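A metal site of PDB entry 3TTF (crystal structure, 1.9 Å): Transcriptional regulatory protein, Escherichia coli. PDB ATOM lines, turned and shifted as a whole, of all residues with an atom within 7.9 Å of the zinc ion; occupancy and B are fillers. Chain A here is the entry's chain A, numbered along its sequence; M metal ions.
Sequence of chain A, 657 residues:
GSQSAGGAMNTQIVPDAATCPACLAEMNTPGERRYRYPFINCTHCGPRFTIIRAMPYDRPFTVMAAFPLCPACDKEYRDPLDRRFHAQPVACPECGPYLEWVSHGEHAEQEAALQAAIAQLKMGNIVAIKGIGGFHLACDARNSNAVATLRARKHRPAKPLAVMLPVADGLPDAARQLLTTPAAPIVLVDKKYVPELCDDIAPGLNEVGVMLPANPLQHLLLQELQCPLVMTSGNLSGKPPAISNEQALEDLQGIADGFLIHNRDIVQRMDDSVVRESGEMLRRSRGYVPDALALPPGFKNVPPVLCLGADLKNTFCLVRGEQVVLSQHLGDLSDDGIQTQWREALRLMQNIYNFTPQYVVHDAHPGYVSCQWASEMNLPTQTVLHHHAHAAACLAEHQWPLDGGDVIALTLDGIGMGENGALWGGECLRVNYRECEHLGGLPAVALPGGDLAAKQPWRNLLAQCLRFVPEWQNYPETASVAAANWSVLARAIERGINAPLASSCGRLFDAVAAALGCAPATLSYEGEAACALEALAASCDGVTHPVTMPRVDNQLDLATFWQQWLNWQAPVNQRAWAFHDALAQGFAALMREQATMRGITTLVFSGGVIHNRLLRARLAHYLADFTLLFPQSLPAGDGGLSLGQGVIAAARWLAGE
Cys 70 touches the zinc ion (SG to ZN, 3.1 Å). Within 4 Å of the zinc ion: Cys 70, Cys 73, Cys 92 and Cys 95. Along chain A the residues within 4 Å of the zinc ion span positions 70 to 95. The nearest printed residue that does not touch the zinc ion is Ala 91 (4.1 Å).
The zinc ion is bound by the side-chain sulfur of Cys 73 (2.1 Å), the side-chain sulfur of Cys 92 (2.4 Å) and the side-chain sulfur of Cys 95 (2.4 Å).
The side-chain sulfur (SG) of Cys 73 lies close to the guanidinium group (NH2) of Arg 33 (2.7 Å). NH1 of Arg 34 sits close to SG of Cys 73, 3.3 Å away. NE of Arg 33 sits close to SG of Cys 92 (3.1 Å). The backbone NH (N) of Glu 94 sits close to the side-chain sulfur (SG) of Cys 92 (3.2 Å). SG of Cys 95 lies close to N of Cys 70 (3.5 Å). The side-chain sulfur (SG) of Cys 70 sits close to the backbone NH (N) of Ala 72, 3.4 Å away.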
ATOM      1  N   ARG A  33     -19.821  -7.057  -6.866  1.00  0.00           N
ATOM      2  CA  ARG A  33     -20.117  -8.496  -6.929  1.00  0.00           C
ATOM      3  C   ARG A  33     -20.137  -9.021  -8.376  1.00  0.00           C
ATOM      4  O   ARG A  33     -19.755 -10.169  -8.644  1.00  0.00           O
ATOM      5  CB  ARG A  33     -21.413  -8.835  -6.184  1.00  0.00           C
ATOM      6  CG  ARG A  33     -21.605 -10.349  -5.954  1.00  0.00           C
ATOM      7  CD  ARG A  33     -22.783 -10.682  -5.057  1.00  0.00           C
ATOM      8  NE  ARG A  33     -24.051 -10.701  -5.784  1.00  0.00           N
ATOM      9  CZ  ARG A  33     -24.892  -9.671  -5.855  1.00  0.00           C
ATOM     10  NH1 ARG A  33     -24.594  -8.523  -5.245  1.00  0.00           N
ATOM     11  NH2 ARG A  33     -26.026  -9.787  -6.529  1.00  0.00           N
ATOM     12  N   ARG A  34     -20.542  -8.163  -9.312  1.00  0.00           N
ATOM     13  CA  ARG A  34     -20.628  -8.544 -10.733  1.00  0.00           C
ATOM     14  C   ARG A  34     -19.424  -8.075 -11.539  1.00  0.00           C
ATOM     15  O   ARG A  34     -19.511  -7.854 -12.757  1.00  0.00           O
ATOM     16  CB  ARG A  34     -21.957  -8.081 -11.342  1.00  0.00           C
ATOM     17  CG  ARG A  34     -23.151  -8.718 -10.677  1.00  0.00           C
ATOM     18  CD  ARG A  34     -24.451  -8.266 -11.255  1.00  0.00           C
ATOM     19  NE  ARG A  34     -25.533  -9.024 -10.626  1.00  0.00           N
ATOM     20  CZ  ARG A  34     -26.304  -8.572  -9.643  1.00  0.00           C
ATOM     21  NH1 ARG A  34     -27.237  -9.366  -9.122  1.00  0.00           N
ATOM     22  NH2 ARG A  34     -26.161  -7.337  -9.178  1.00  0.00           N
ATOM     23  N   TYR A  37     -18.473 -10.171 -14.640  1.00  0.00           N
ATOM     24  CA  TYR A  37     -19.525 -11.177 -14.780  1.00  0.00           C
ATOM     25  C   TYR A  37     -20.143 -11.006 -16.175  1.00  0.00           C
ATOM     26  O   TYR A  37     -20.742  -9.963 -16.468  1.00  0.00           O
ATOM     27  CB  TYR A  37     -20.539 -11.035 -13.629  1.00  0.00           C
ATOM     28  CG  TYR A  37     -21.768 -11.916 -13.670  1.00  0.00           C
ATOM     29  CD1 TYR A  37     -21.676 -13.309 -13.742  1.00  0.00           C
ATOM     30  CD2 TYR A  37     -23.046 -11.355 -13.594  1.00  0.00           C
ATOM     31  CE1 TYR A  37     -22.825 -14.107 -13.775  1.00  0.00           C
ATOM     32  CE2 TYR A  37     -24.190 -12.141 -13.609  1.00  0.00           C
ATOM     33  CZ  TYR A  37     -24.072 -13.508 -13.700  1.00  0.00           C
ATOM     34  OH  TYR A  37     -25.223 -14.274 -13.727  1.00  0.00           O
ATOM     35  N   ARG A  59     -39.282 -14.778 -14.069  1.00  0.00           N
ATOM     36  CA  ARG A  59     -38.225 -15.773 -13.875  1.00  0.00           C
ATOM     37  C   ARG A  59     -38.669 -17.246 -14.079  1.00  0.00           C
ATOM     38  O   ARG A  59     -38.012 -17.962 -14.827  1.00  0.00           O
ATOM     39  CB  ARG A  59     -37.494 -15.569 -12.533  1.00  0.00           C
ATOM     40  CG  ARG A  59     -36.219 -16.406 -12.381  1.00  0.00           C
ATOM     41  CD  ARG A  59     -35.388 -16.073 -11.135  1.00  0.00           C
ATOM     42  NE  ARG A  59     -33.979 -16.467 -11.310  1.00  0.00           N
ATOM     43  CZ  ARG A  59     -33.051 -15.713 -11.891  1.00  0.00           C
ATOM     44  NH1 ARG A  59     -33.362 -14.508 -12.353  1.00  0.00           N
ATOM     45  NH2 ARG A  59     -31.806 -16.161 -12.015  1.00  0.00           N
ATOM     46  N   PHE A  67     -31.833 -20.836 -12.416  1.00  0.00           N
ATOM     47  CA  PHE A  67     -30.837 -20.193 -11.563  1.00  0.00           C
ATOM     48  C   PHE A  67     -31.507 -19.395 -10.441  1.00  0.00           C
ATOM     49  O   PHE A  67     -31.612 -18.169 -10.523  1.00  0.00           O
ATOM     50  CB  PHE A  67     -29.912 -19.265 -12.386  1.00  0.00           C
ATOM     51  CG  PHE A  67     -29.204 -19.963 -13.525  1.00  0.00           C
ATOM     52  CD1 PHE A  67     -27.965 -20.579 -13.319  1.00  0.00           C
ATOM     53  CD2 PHE A  67     -29.772 -20.007 -14.794  1.00  0.00           C
ATOM     54  CE1 PHE A  67     -27.306 -21.233 -14.376  1.00  0.00           C
ATOM     55  CE2 PHE A  67     -29.117 -20.663 -15.860  1.00  0.00           C
ATOM     56  CZ  PHE A  67     -27.883 -21.269 -15.653  1.00  0.00           C
ATOM     57  N   PRO A  68     -31.974 -20.083  -9.371  1.00  0.00           N
ATOM     58  CA  PRO A  68     -32.583 -19.345  -8.252  1.00  0.00           C
ATOM     59  C   PRO A  68     -31.603 -18.343  -7.642  1.00  0.00           C
ATOM     60  O   PRO A  68     -30.411 -18.634  -7.524  1.00  0.00           O
ATOM     61  CB  PRO A  68     -32.941 -20.453  -7.257  1.00  0.00           C
ATOM     62  CG  PRO A  68     -33.070 -21.692  -8.085  1.00  0.00           C
ATOM     63  CD  PRO A  68     -31.984 -21.533  -9.120  1.00  0.00           C
ATOM     64  N   LEU A  69     -32.111 -17.156  -7.292  1.00  0.00           N
ATOM     65  CA  LEU A  69     -31.240 -16.063  -6.856  1.00  0.00           C
ATOM     66  C   LEU A  69     -30.636 -16.372  -5.500  1.00  0.00           C
ATOM     67  O   LEU A  69     -31.368 -16.735  -4.574  1.00  0.00           O
ATOM     68  CB  LEU A  69     -32.017 -14.750  -6.780  1.00  0.00           C
ATOM     69  CG  LEU A  69     -32.493 -14.095  -8.074  1.00  0.00           C
ATOM     70  CD1 LEU A  69     -33.333 -12.866  -7.755  1.00  0.00           C
ATOM     71  CD2 LEU A  69     -31.309 -13.732  -8.920  1.00  0.00           C
ATOM     72  N   CYS A  70     -29.326 -16.222  -5.390  1.00  0.00           N
ATOM     73  CA  CYS A  70     -28.686 -16.304  -4.084  1.00  0.00           C
ATOM     74  C   CYS A  70     -29.175 -15.139  -3.209  1.00  0.00           C
ATOM     75  O   CYS A  70     -29.647 -14.127  -3.751  1.00  0.00           O
ATOM     76  CB  CYS A  70     -27.155 -16.306  -4.225  1.00  0.00           C
ATOM     77  SG  CYS A  70     -26.378 -14.664  -4.160  1.00  0.00           S
ATOM     78  N   PRO A  71     -29.092 -15.276  -1.872  1.00  0.00           N
ATOM     79  CA  PRO A  71     -29.484 -14.193  -0.948  1.00  0.00           C
ATOM     80  C   PRO A  71     -28.979 -12.771  -1.271  1.00  0.00           C
ATOM     81  O   PRO A  71     -29.711 -11.800  -1.067  1.00  0.00           O
ATOM     82  CB  PRO A  71     -28.943 -14.688   0.397  1.00  0.00           C
ATOM     83  CG  PRO A  71     -29.041 -16.180   0.282  1.00  0.00           C
ATOM     84  CD  PRO A  71     -28.678 -16.485  -1.153  1.00  0.00           C
ATOM     85  N   ALA A  72     -27.748 -12.662  -1.781  1.00  0.00           N
ATOM     86  CA  ALA A  72     -27.194 -11.356  -2.149  1.00  0.00           C
ATOM     87  C   ALA A  72     -27.975 -10.637  -3.268  1.00  0.00           C
ATOM     88  O   ALA A  72     -28.261  -9.448  -3.138  1.00  0.00           O
ATOM     89  CB  ALA A  72     -25.718 -11.481  -2.507  1.00  0.00           C
ATOM     90  N   CYS A  73     -28.296 -11.357  -4.343  1.00  0.00           N
ATOM     91  CA  CYS A  73     -29.076 -10.793  -5.471  1.00  0.00           C
ATOM     92  C   CYS A  73     -30.549 -10.622  -5.111  1.00  0.00           C
ATOM     93  O   CYS A  73     -31.224  -9.752  -5.671  1.00  0.00           O
ATOM     94  CB  CYS A  73     -28.981 -11.656  -6.728  1.00  0.00           C
ATOM     95  SG  CYS A  73     -27.338 -12.077  -7.301  1.00  0.00           S
ATOM     96  N   ASP A  74     -31.021 -11.473  -4.199  1.00  0.00           N
ATOM     97  CA  ASP A  74     -32.395 -11.428  -3.688  1.00  0.00           C
ATOM     98  C   ASP A  74     -32.732 -10.053  -3.097  1.00  0.00           C
ATOM     99  O   ASP A  74     -33.793  -9.486  -3.379  1.00  0.00           O
ATOM    100  CB  ASP A  74     -32.606 -12.538  -2.640  1.00  0.00           C
ATOM    101  CG  ASP A  74     -33.969 -13.229  -2.752  1.00  0.00           C
ATOM    102  OD1 ASP A  74     -34.714 -12.982  -3.727  1.00  0.00           O
ATOM    103  OD2 ASP A  74     -34.284 -14.045  -1.858  1.00  0.00           O
ATOM    104  N   GLU A  76     -31.493  -7.251  -3.934  1.00  0.00           N
ATOM    105  CA  GLU A  76     -31.540  -6.276  -5.014  1.00  0.00           C
ATOM    106  C   GLU A  76     -32.853  -6.321  -5.804  1.00  0.00           C
ATOM    107  O   GLU A  76     -33.397  -5.273  -6.190  1.00  0.00           O
ATOM    108  CB  GLU A  76     -30.342  -6.467  -5.949  1.00  0.00           C
ATOM    109  CG  GLU A  76     -29.002  -6.193  -5.275  1.00  0.00           C
ATOM    110  CD  GLU A  76     -27.822  -6.798  -6.019  1.00  0.00           C
ATOM    111  OE1 GLU A  76     -28.039  -7.621  -6.938  1.00  0.00           O
ATOM    112  OE2 GLU A  76     -26.678  -6.458  -5.664  1.00  0.00           O
ATOM    113  N   VAL A  90     -31.194 -10.913 -13.909  1.00  0.00           N
ATOM    114  CA  VAL A  90     -30.306 -10.522 -12.803  1.00  0.00           C
ATOM    115  C   VAL A  90     -29.227 -11.605 -12.535  1.00  0.00           C
ATOM    116  O   VAL A  90     -28.600 -12.075 -13.487  1.00  0.00           O
ATOM    117  CB  VAL A  90     -31.119 -10.005 -11.521  1.00  0.00           C
ATOM    118  CG1 VAL A  90     -32.006 -11.091 -10.906  1.00  0.00           C
ATOM    119  CG2 VAL A  90     -30.207  -9.373 -10.471  1.00  0.00           C
ATOM    120  N   ALA A  91     -29.017 -12.004 -11.290  1.00  0.00           N
ATOM    121  CA  ALA A  91     -27.989 -13.003 -10.911  1.00  0.00           C
ATOM    122  C   ALA A  91     -26.562 -12.423 -10.914  1.00  0.00           C
ATOM    123  O   ALA A  91     -26.337 -11.301 -11.380  1.00  0.00           O
ATOM    124  CB  ALA A  91     -28.101 -14.274 -11.780  1.00  0.00           C
ATOM    125  N   CYS A  92     -25.619 -13.202 -10.380  1.00  0.00           N
ATOM    126  CA  CYS A  92     -24.230 -12.780 -10.166  1.00  0.00           C
ATOM    127  C   CYS A  92     -23.334 -14.013 -10.317  1.00  0.00           C
ATOM    128  O   CYS A  92     -23.856 -15.099 -10.600  1.00  0.00           O
ATOM    129  CB  CYS A  92     -24.066 -12.178  -8.760  1.00  0.00           C
ATOM    130  SG  CYS A  92     -24.039 -13.412  -7.386  1.00  0.00           S
ATOM    131  N   PRO A  93     -21.999 -13.871 -10.138  1.00  0.00           N
ATOM    132  CA  PRO A  93     -21.121 -15.041 -10.243  1.00  0.00           C
ATOM    133  C   PRO A  93     -21.420 -16.158  -9.211  1.00  0.00           C
ATOM    134  O   PRO A  93     -21.065 -17.323  -9.435  1.00  0.00           O
ATOM    135  CB  PRO A  93     -19.714 -14.453 -10.021  1.00  0.00           C
ATOM    136  CG  PRO A  93     -19.851 -12.984 -10.292  1.00  0.00           C
ATOM    137  CD  PRO A  93     -21.236 -12.633  -9.851  1.00  0.00           C
ATOM    138  N   GLU A  94     -22.059 -15.803  -8.101  1.00  0.00           N
ATOM    139  CA  GLU A  94     -22.449 -16.783  -7.085  1.00  0.00           C
ATOM    140  C   GLU A  94     -23.589 -17.719  -7.503  1.00  0.00           C
ATOM    141  O   GLU A  94     -23.565 -18.903  -7.178  1.00  0.00           O
ATOM    142  CB  GLU A  94     -22.750 -16.111  -5.741  1.00  0.00           C
ATOM    143  CG  GLU A  94     -21.576 -16.124  -4.773  1.00  0.00           C
ATOM    144  CD  GLU A  94     -20.476 -15.132  -5.146  1.00  0.00           C
ATOM    145  OE1 GLU A  94     -19.484 -15.562  -5.782  1.00  0.00           O
ATOM    146  OE2 GLU A  94     -20.590 -13.929  -4.803  1.00  0.00           O
ATOM    147  N   CYS A  95     -24.571 -17.192  -8.241  1.00  0.00           N
ATOM    148  CA  CYS A  95     -25.776 -17.970  -8.564  1.00  0.00           C
ATOM    149  C   CYS A  95     -26.115 -18.075 -10.057  1.00  0.00           C
ATOM    150  O   CYS A  95     -26.994 -18.854 -10.437  1.00  0.00           O
ATOM    151  CB  CYS A  95     -26.973 -17.424  -7.776  1.00  0.00           C
ATOM    152  SG  CYS A  95     -27.502 -15.780  -8.301  1.00  0.00           S
ATOM    153  N   GLY A  96     -25.424 -17.294 -10.890  1.00  0.00           N
ATOM    154  CA  GLY A  96     -25.763 -17.205 -12.322  1.00  0.00           C
ATOM    155  C   GLY A  96     -25.171 -18.242 -13.270  1.00  0.00           C
ATOM    156  O   GLY A  96     -24.556 -19.228 -12.832  1.00  0.00           O
HETATM  157 ZN    ZN M   1     -26.388 -13.951  -7.136  1.00  0.00          ZN
